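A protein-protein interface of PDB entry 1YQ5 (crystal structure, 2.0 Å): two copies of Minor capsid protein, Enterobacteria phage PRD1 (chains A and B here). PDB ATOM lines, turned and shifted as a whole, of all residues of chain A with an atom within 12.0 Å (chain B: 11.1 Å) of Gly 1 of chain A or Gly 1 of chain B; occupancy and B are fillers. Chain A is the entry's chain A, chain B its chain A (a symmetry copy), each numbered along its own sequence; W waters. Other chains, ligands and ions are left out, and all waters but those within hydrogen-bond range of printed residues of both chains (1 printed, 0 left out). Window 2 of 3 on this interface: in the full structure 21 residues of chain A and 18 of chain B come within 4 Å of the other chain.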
ATOM      1  N   GLY A   1      17.206  32.743   3.432  1.00  0.00           N
ATOM      2  CA  GLY A   1      17.015  32.503   4.901  1.00  0.00           C
ATOM      3  C   GLY A   1      15.548  32.353   5.259  1.00  0.00           C
ATOM      4  O   GLY A   1      14.703  33.128   4.798  1.00  0.00           O
ATOM      5  N   GLY A   2      15.243  31.363   6.090  1.00  0.00           N
ATOM      6  CA  GLY A   2      13.866  31.125   6.491  1.00  0.00           C
ATOM      7  C   GLY A   2      13.214  30.131   5.553  1.00  0.00           C
ATOM      8  O   GLY A   2      13.862  29.624   4.632  1.00  0.00           O
ATOM      9  N   VAL A   3      11.933  29.851   5.767  1.00  0.00           N
ATOM     10  CA  VAL A   3      11.220  28.901   4.921  1.00  0.00           C
ATOM     11  C   VAL A   3      10.130  29.621   4.137  1.00  0.00           C
ATOM     12  O   VAL A   3       9.663  30.690   4.539  1.00  0.00           O
ATOM     13  CB  VAL A   3      10.591  27.777   5.769  1.00  0.00           C
ATOM     14  CG1 VAL A   3      11.668  27.093   6.595  1.00  0.00           C
ATOM     15  CG2 VAL A   3       9.516  28.342   6.675  1.00  0.00           C
ATOM     16  N   THR A   4       9.721  29.034   3.020  1.00  0.00           N
ATOM     17  CA  THR A   4       8.697  29.644   2.176  1.00  0.00           C
ATOM     18  C   THR A   4       7.287  29.429   2.714  1.00  0.00           C
ATOM     19  O   THR A   4       6.421  30.296   2.573  1.00  0.00           O
ATOM     20  CB  THR A   4       8.758  29.078   0.749  1.00  0.00           C
ATOM     21  OG1 THR A   4       8.471  27.677   0.781  1.00  0.00           O
ATOM     22  CG2 THR A   4      10.147  29.288   0.154  1.00  0.00           C
ATOM     23  N   ASP A   5       7.055  28.273   3.324  1.00  0.00           N
ATOM     24  CA  ASP A   5       5.742  27.960   3.863  1.00  0.00           C
ATOM     25  C   ASP A   5       5.837  27.212   5.178  1.00  0.00           C
ATOM     26  O   ASP A   5       6.704  26.358   5.360  1.00  0.00           O
ATOM     27  CB  ASP A   5       4.947  27.117   2.866  1.00  0.00           C
ATOM     28  CG  ASP A   5       4.872  27.759   1.501  1.00  0.00           C
ATOM     29  OD1 ASP A   5       5.837  27.619   0.722  1.00  0.00           O
ATOM     30  OD2 ASP A   5       3.851  28.414   1.217  1.00  0.00           O
ATOM     31  N   ALA A   6       4.931  27.539   6.092  1.00  0.00           N
ATOM     32  CA  ALA A   6       4.900  26.891   7.395  1.00  0.00           C
ATOM     33  C   ALA A   6       3.567  27.162   8.063  1.00  0.00           C
ATOM     34  O   ALA A   6       2.894  28.154   7.766  1.00  0.00           O
ATOM     35  CB  ALA A   6       6.040  27.408   8.274  1.00  0.00           C
ATOM     36  N   VAL A  40       3.199  30.977   7.732  1.00  0.00           N
ATOM     37  CA  VAL A  40       4.155  31.573   6.805  1.00  0.00           C
ATOM     38  C   VAL A  40       3.767  31.175   5.386  1.00  0.00           C
ATOM     39  O   VAL A  40       3.607  29.991   5.086  1.00  0.00           O
ATOM     40  CB  VAL A  40       5.591  31.084   7.090  1.00  0.00           C
ATOM     41  CG1 VAL A  40       6.561  31.692   6.084  1.00  0.00           C
ATOM     42  CG2 VAL A  40       5.995  31.463   8.509  1.00  0.00           C
ATOM     43  N   GLY A  41       3.609  32.165   4.513  1.00  0.00           N
ATOM     44  CA  GLY A  41       3.233  31.871   3.142  1.00  0.00           C
ATOM     45  C   GLY A  41       1.813  31.340   3.084  1.00  0.00           C
ATOM     46  O   GLY A  41       1.062  31.462   4.049  1.00  0.00           O
ATOM     47  N   ALA A 141       6.636  22.659   8.095  1.00  0.00           N
ATOM     48  CA  ALA A 141       7.357  23.683   7.357  1.00  0.00           C
ATOM     49  C   ALA A 141       8.001  23.077   6.123  1.00  0.00           C
ATOM     50  O   ALA A 141       8.594  22.000   6.186  1.00  0.00           O
ATOM     51  CB  ALA A 141       8.426  24.323   8.242  1.00  0.00           C
ATOM     52  N   LYS A 142       7.861  23.766   4.995  1.00  0.00           N
ATOM     53  CA  LYS A 142       8.453  23.315   3.745  1.00  0.00           C
ATOM     54  C   LYS A 142       9.889  23.818   3.781  1.00  0.00           C
ATOM     55  O   LYS A 142      10.114  25.027   3.749  1.00  0.00           O
ATOM     56  CB  LYS A 142       7.709  23.936   2.562  1.00  0.00           C
ATOM     57  CG  LYS A 142       8.185  23.474   1.190  1.00  0.00           C
ATOM     58  CD  LYS A 142       7.377  24.138   0.084  1.00  0.00           C
ATOM     59  CE  LYS A 142       7.728  23.576  -1.282  1.00  0.00           C
ATOM     60  NZ  LYS A 142       9.165  23.774  -1.606  1.00  0.00           N
ATOM     61  N   ILE A 143      10.861  22.912   3.858  1.00  0.00           N
ATOM     62  CA  ILE A 143      12.253  23.350   3.916  1.00  0.00           C
ATOM     63  C   ILE A 143      12.987  23.323   2.579  1.00  0.00           C
ATOM     64  O   ILE A 143      14.134  23.753   2.494  1.00  0.00           O
ATOM     65  CB  ILE A 143      13.071  22.545   4.951  1.00  0.00           C
ATOM     66  CG1 ILE A 143      13.292  21.121   4.458  1.00  0.00           C
ATOM     67  CG2 ILE A 143      12.342  22.535   6.296  1.00  0.00           C
ATOM     68  CD1 ILE A 143      14.366  20.396   5.236  1.00  0.00           C
ATOM     69  N   ASN A 144      12.338  22.805   1.542  1.00  0.00           N
ATOM     70  CA  ASN A 144      12.931  22.786   0.203  1.00  0.00           C
ATOM     71  C   ASN A 144      11.850  22.538  -0.834  1.00  0.00           C
ATOM     72  O   ASN A 144      12.024  22.990  -1.983  1.00  0.00           O
ATOM     73  CB  ASN A 144      14.013  21.712   0.061  1.00  0.00           C
ATOM     74  CG  ASN A 144      14.869  21.919  -1.190  1.00  0.00           C
ATOM     75  OD1 ASN A 144      15.576  22.920  -1.311  1.00  0.00           O
ATOM     76  ND2 ASN A 144      14.791  20.983  -2.128  1.00  0.00           N
ATOM     77  OXT ASN A 144      10.853  21.876  -0.479  1.00  0.00           O
ATOM     78  N   GLY B   1      20.264  30.601   2.042  1.00  0.00           N
ATOM     79  CA  GLY B   1      20.768  29.228   2.376  1.00  0.00           C
ATOM     80  C   GLY B   1      21.383  29.179   3.762  1.00  0.00           C
ATOM     81  O   GLY B   1      22.156  30.066   4.143  1.00  0.00           O
ATOM     82  N   GLY B   2      21.053  28.137   4.517  1.00  0.00           N
ATOM     83  CA  GLY B   2      21.580  27.997   5.864  1.00  0.00           C
ATOM     84  C   GLY B   2      20.635  28.632   6.862  1.00  0.00           C
ATOM     85  O   GLY B   2      19.573  29.136   6.483  1.00  0.00           O
ATOM     86  N   VAL B   3      21.010  28.624   8.137  1.00  0.00           N
ATOM     87  CA  VAL B   3      20.164  29.205   9.173  1.00  0.00           C
ATOM     88  C   VAL B   3      20.852  30.419   9.784  1.00  0.00           C
ATOM     89  O   VAL B   3      22.078  30.548   9.726  1.00  0.00           O
ATOM     90  CB  VAL B   3      19.861  28.171  10.277  1.00  0.00           C
ATOM     91  CG1 VAL B   3      19.225  26.936   9.663  1.00  0.00           C
ATOM     92  CG2 VAL B   3      21.134  27.798  11.009  1.00  0.00           C
ATOM     93  N   THR B   4      20.065  31.309  10.373  1.00  0.00           N
ATOM     94  CA  THR B   4      20.612  32.523  10.974  1.00  0.00           C
ATOM     95  C   THR B   4      21.229  32.275  12.345  1.00  0.00           C
ATOM     96  O   THR B   4      22.219  32.910  12.713  1.00  0.00           O
ATOM     97  CB  THR B   4      19.522  33.597  11.124  1.00  0.00           C
ATOM     98  OG1 THR B   4      18.511  33.124  12.020  1.00  0.00           O
ATOM     99  CG2 THR B   4      18.886  33.899   9.771  1.00  0.00           C
ATOM    100  N   ASP B   5      20.640  31.356  13.101  1.00  0.00           N
ATOM    101  CA  ASP B   5      21.139  31.050  14.433  1.00  0.00           C
ATOM    102  C   ASP B   5      21.051  29.567  14.739  1.00  0.00           C
ATOM    103  O   ASP B   5      20.088  28.900  14.364  1.00  0.00           O
ATOM    104  CB  ASP B   5      20.349  31.825  15.486  1.00  0.00           C
ATOM    105  CG  ASP B   5      20.321  33.310  15.209  1.00  0.00           C
ATOM    106  OD1 ASP B   5      19.492  33.747  14.385  1.00  0.00           O
ATOM    107  OD2 ASP B   5      21.141  34.032  15.806  1.00  0.00           O
ATOM    108  N   ALA B   6      22.066  29.063  15.429  1.00  0.00           N
ATOM    109  CA  ALA B   6      22.105  27.656  15.801  1.00  0.00           C
ATOM    110  C   ALA B   6      23.141  27.448  16.888  1.00  0.00           C
ATOM    111  O   ALA B   6      24.090  28.226  17.022  1.00  0.00           O
ATOM    112  CB  ALA B   6      22.442  26.792  14.585  1.00  0.00           C
ATOM    113  N   VAL B  40      26.248  29.211  15.460  1.00  0.00           N
ATOM    114  CA  VAL B  40      25.957  30.051  14.304  1.00  0.00           C
ATOM    115  C   VAL B  40      25.187  31.278  14.777  1.00  0.00           C
ATOM    116  O   VAL B  40      24.162  31.157  15.449  1.00  0.00           O
ATOM    117  CB  VAL B  40      25.106  29.295  13.261  1.00  0.00           C
ATOM    118  CG1 VAL B  40      24.787  30.207  12.084  1.00  0.00           C
ATOM    119  CG2 VAL B  40      25.855  28.057  12.783  1.00  0.00           C
ATOM    120  N   LYS B  57      14.148  37.334  18.474  1.00  0.00           N
ATOM    121  CA  LYS B  57      14.315  36.065  17.771  1.00  0.00           C
ATOM    122  C   LYS B  57      13.099  35.133  17.747  1.00  0.00           C
ATOM    123  O   LYS B  57      13.258  33.915  17.728  1.00  0.00           O
ATOM    124  CB  LYS B  57      15.522  35.307  18.343  1.00  0.00           C
ATOM    125  CG  LYS B  57      16.878  35.974  18.086  1.00  0.00           C
ATOM    126  CD  LYS B  57      17.257  35.932  16.610  1.00  0.00           C
ATOM    127  CE  LYS B  57      18.565  36.670  16.338  1.00  0.00           C
ATOM    128  NZ  LYS B  57      18.968  36.553  14.898  1.00  0.00           N
ATOM    129  N   LEU B  60      10.484  29.882  14.230  1.00  0.00           N
ATOM    130  CA  LEU B  60      10.445  28.427  14.255  1.00  0.00           C
ATOM    131  C   LEU B  60      11.816  27.872  14.592  1.00  0.00           C
ATOM    132  O   LEU B  60      12.828  28.295  14.025  1.00  0.00           O
ATOM    133  CB  LEU B  60       9.992  27.887  12.897  1.00  0.00           C
ATOM    134  CG  LEU B  60       8.544  28.191  12.508  1.00  0.00           C
ATOM    135  CD1 LEU B  60       8.306  27.807  11.055  1.00  0.00           C
ATOM    136  CD2 LEU B  60       7.598  27.420  13.431  1.00  0.00           C
ATOM    137  N   LYS B 142      17.364  28.032  14.506  1.00  0.00           N
ATOM    138  CA  LYS B 142      16.231  28.868  14.138  1.00  0.00           C
ATOM    139  C   LYS B 142      16.081  28.695  12.634  1.00  0.00           C
ATOM    140  O   LYS B 142      16.960  29.112  11.881  1.00  0.00           O
ATOM    141  CB  LYS B 142      16.531  30.329  14.472  1.00  0.00           C
ATOM    142  CG  LYS B 142      15.383  31.297  14.208  1.00  0.00           C
ATOM    143  CD  LYS B 142      15.777  32.719  14.581  1.00  0.00           C
ATOM    144  CE  LYS B 142      14.601  33.674  14.475  1.00  0.00           C
ATOM    145  NZ  LYS B 142      14.050  33.715  13.095  1.00  0.00           N
ATOM    146  N   ILE B 143      14.989  28.080  12.186  1.00  0.00           N
ATOM    147  CA  ILE B 143      14.813  27.873  10.751  1.00  0.00           C
ATOM    148  C   ILE B 143      13.931  28.910  10.061  1.00  0.00           C
ATOM    149  O   ILE B 143      13.787  28.885   8.842  1.00  0.00           O
ATOM    150  CB  ILE B 143      14.271  26.462  10.430  1.00  0.00           C
ATOM    151  CG1 ILE B 143      12.817  26.343  10.866  1.00  0.00           C
ATOM    152  CG2 ILE B 143      15.125  25.405  11.133  1.00  0.00           C
ATOM    153  CD1 ILE B 143      12.129  25.137  10.272  1.00  0.00           C
ATOM    154  N   ASN B 144      13.330  29.806  10.835  1.00  0.00           N
ATOM    155  CA  ASN B 144      12.510  30.877  10.267  1.00  0.00           C
ATOM    156  C   ASN B 144      12.300  31.968  11.302  1.00  0.00           C
ATOM    157  O   ASN B 144      12.111  33.132  10.898  1.00  0.00           O
ATOM    158  CB  ASN B 144      11.144  30.374   9.790  1.00  0.00           C
ATOM    159  CG  ASN B 144      10.440  31.390   8.888  1.00  0.00           C
ATOM    160  OD1 ASN B 144      10.920  31.703   7.797  1.00  0.00           O
ATOM    161  ND2 ASN B 144       9.313  31.917   9.349  1.00  0.00           N
ATOM    162  OXT ASN B 144      12.311  31.631  12.503  1.00  0.00           O
HETATM  163  O   HOH W   1      17.191  29.967   7.316  1.00  0.00           O
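The backbone NH of Val 3 of chain A sits at hydrogen-bond distance from the side-chain amide oxygen of Asn 144 of chain B, 2.9 Å away.
The backbone carbonyl oxygen (O) of Ala 6 of chain A is in hydrogen-bond range of the backbone NH (N) of Val 40 of chain A, at 2.8 Å.
The backbone carbonyl oxygen (O) of Leu 60 of chain B is in hydrogen-bond range of the backbone NH (N) of Ile 143 of chain B (2.8 Å).
The chain-end carboxylate (OXT) of Asn 144 of chain B sits at hydrogen-bond distance from the backbone NH (N) of Leu 60 of chain B (3.1 Å).
OXT of Asn 144 of chain B lies within salt-bridge range of NZ of Lys 142 of chain B, at 2.8 Å.
N of Gly 1 of chain A touches N of Gly 1 of chain B, at 3.98 Å.
Ile 143 of chain B touches Gly 2 of chain A (O to CA, 3.2 Å).
Asn 144 of chain B touches Gly 2 of chain A.
CG1 of Val 3 of chain A touches O of Ile 143 of chain B, at 3.6 Å.
Ala 6 of chain A touches Leu 60 of chain B (CB to CD1, 3.6 Å).
ND2 of Asn 144 of chain B touches CG2 of Val 40 of chain A (3.5 Å).
Of the printed residues of chain B, Gly 1 of chain A touches Gly 1.
Of the printed residues of chain A, Gly 1 of chain B touches Gly 1.
No residue of chain A comes within 4 Å of Val 3 of chain B.
Of the printed residues of chain A, Ile 143 of chain B touches Gly 2 and Val 3.
Of the printed residues of chain A, Leu 60 of chain B touches Ala 6 (3.6 Å).
Printed residues of chain B within 4 Å of Ala 6 of chain A: Leu 60 (3.6 Å).
The nearest printed residue of chain B that does not touch Gly 1 of chain A is Gly 2 of chain B (4.5 Å).
Hydrophobic or aromatic side chains of chain B that line the printed part of chain A: Leu 60.
Among the printed residues, no Asp or Glu carboxylate lies within 4 Å of a Lys or Arg side-chain nitrogen of the other chain.
Gly 1 of chain A touches its own counterpart, Gly 1 of chain B.
Gly 2 of chain A touches Asn 144 of chain B, but with the chains exchanged Asn 144 of chain A does not touch Gly 2 of chain B (9.5 Å).
Val 3 of chain A touches Ile 143 of chain B, but with the chains exchanged Ile 143 of chain A does not touch Val 3 of chain B (8.8 Å).
Val 3 of chain A touches Asn 144 of chain B, but with the chains exchanged Asn 144 of chain A does not touch Val 3 of chain B (11.4 Å).
10 positions are printed for both chains.
Of the 7 pairs that touch across the chains among the printed residues, 1 has its exchanged pair printed and touching as well.
Water W1 bridges O of Gly 2 of chain B (2.7 Å) and N of Gly 2 of chain A (2.7 Å).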
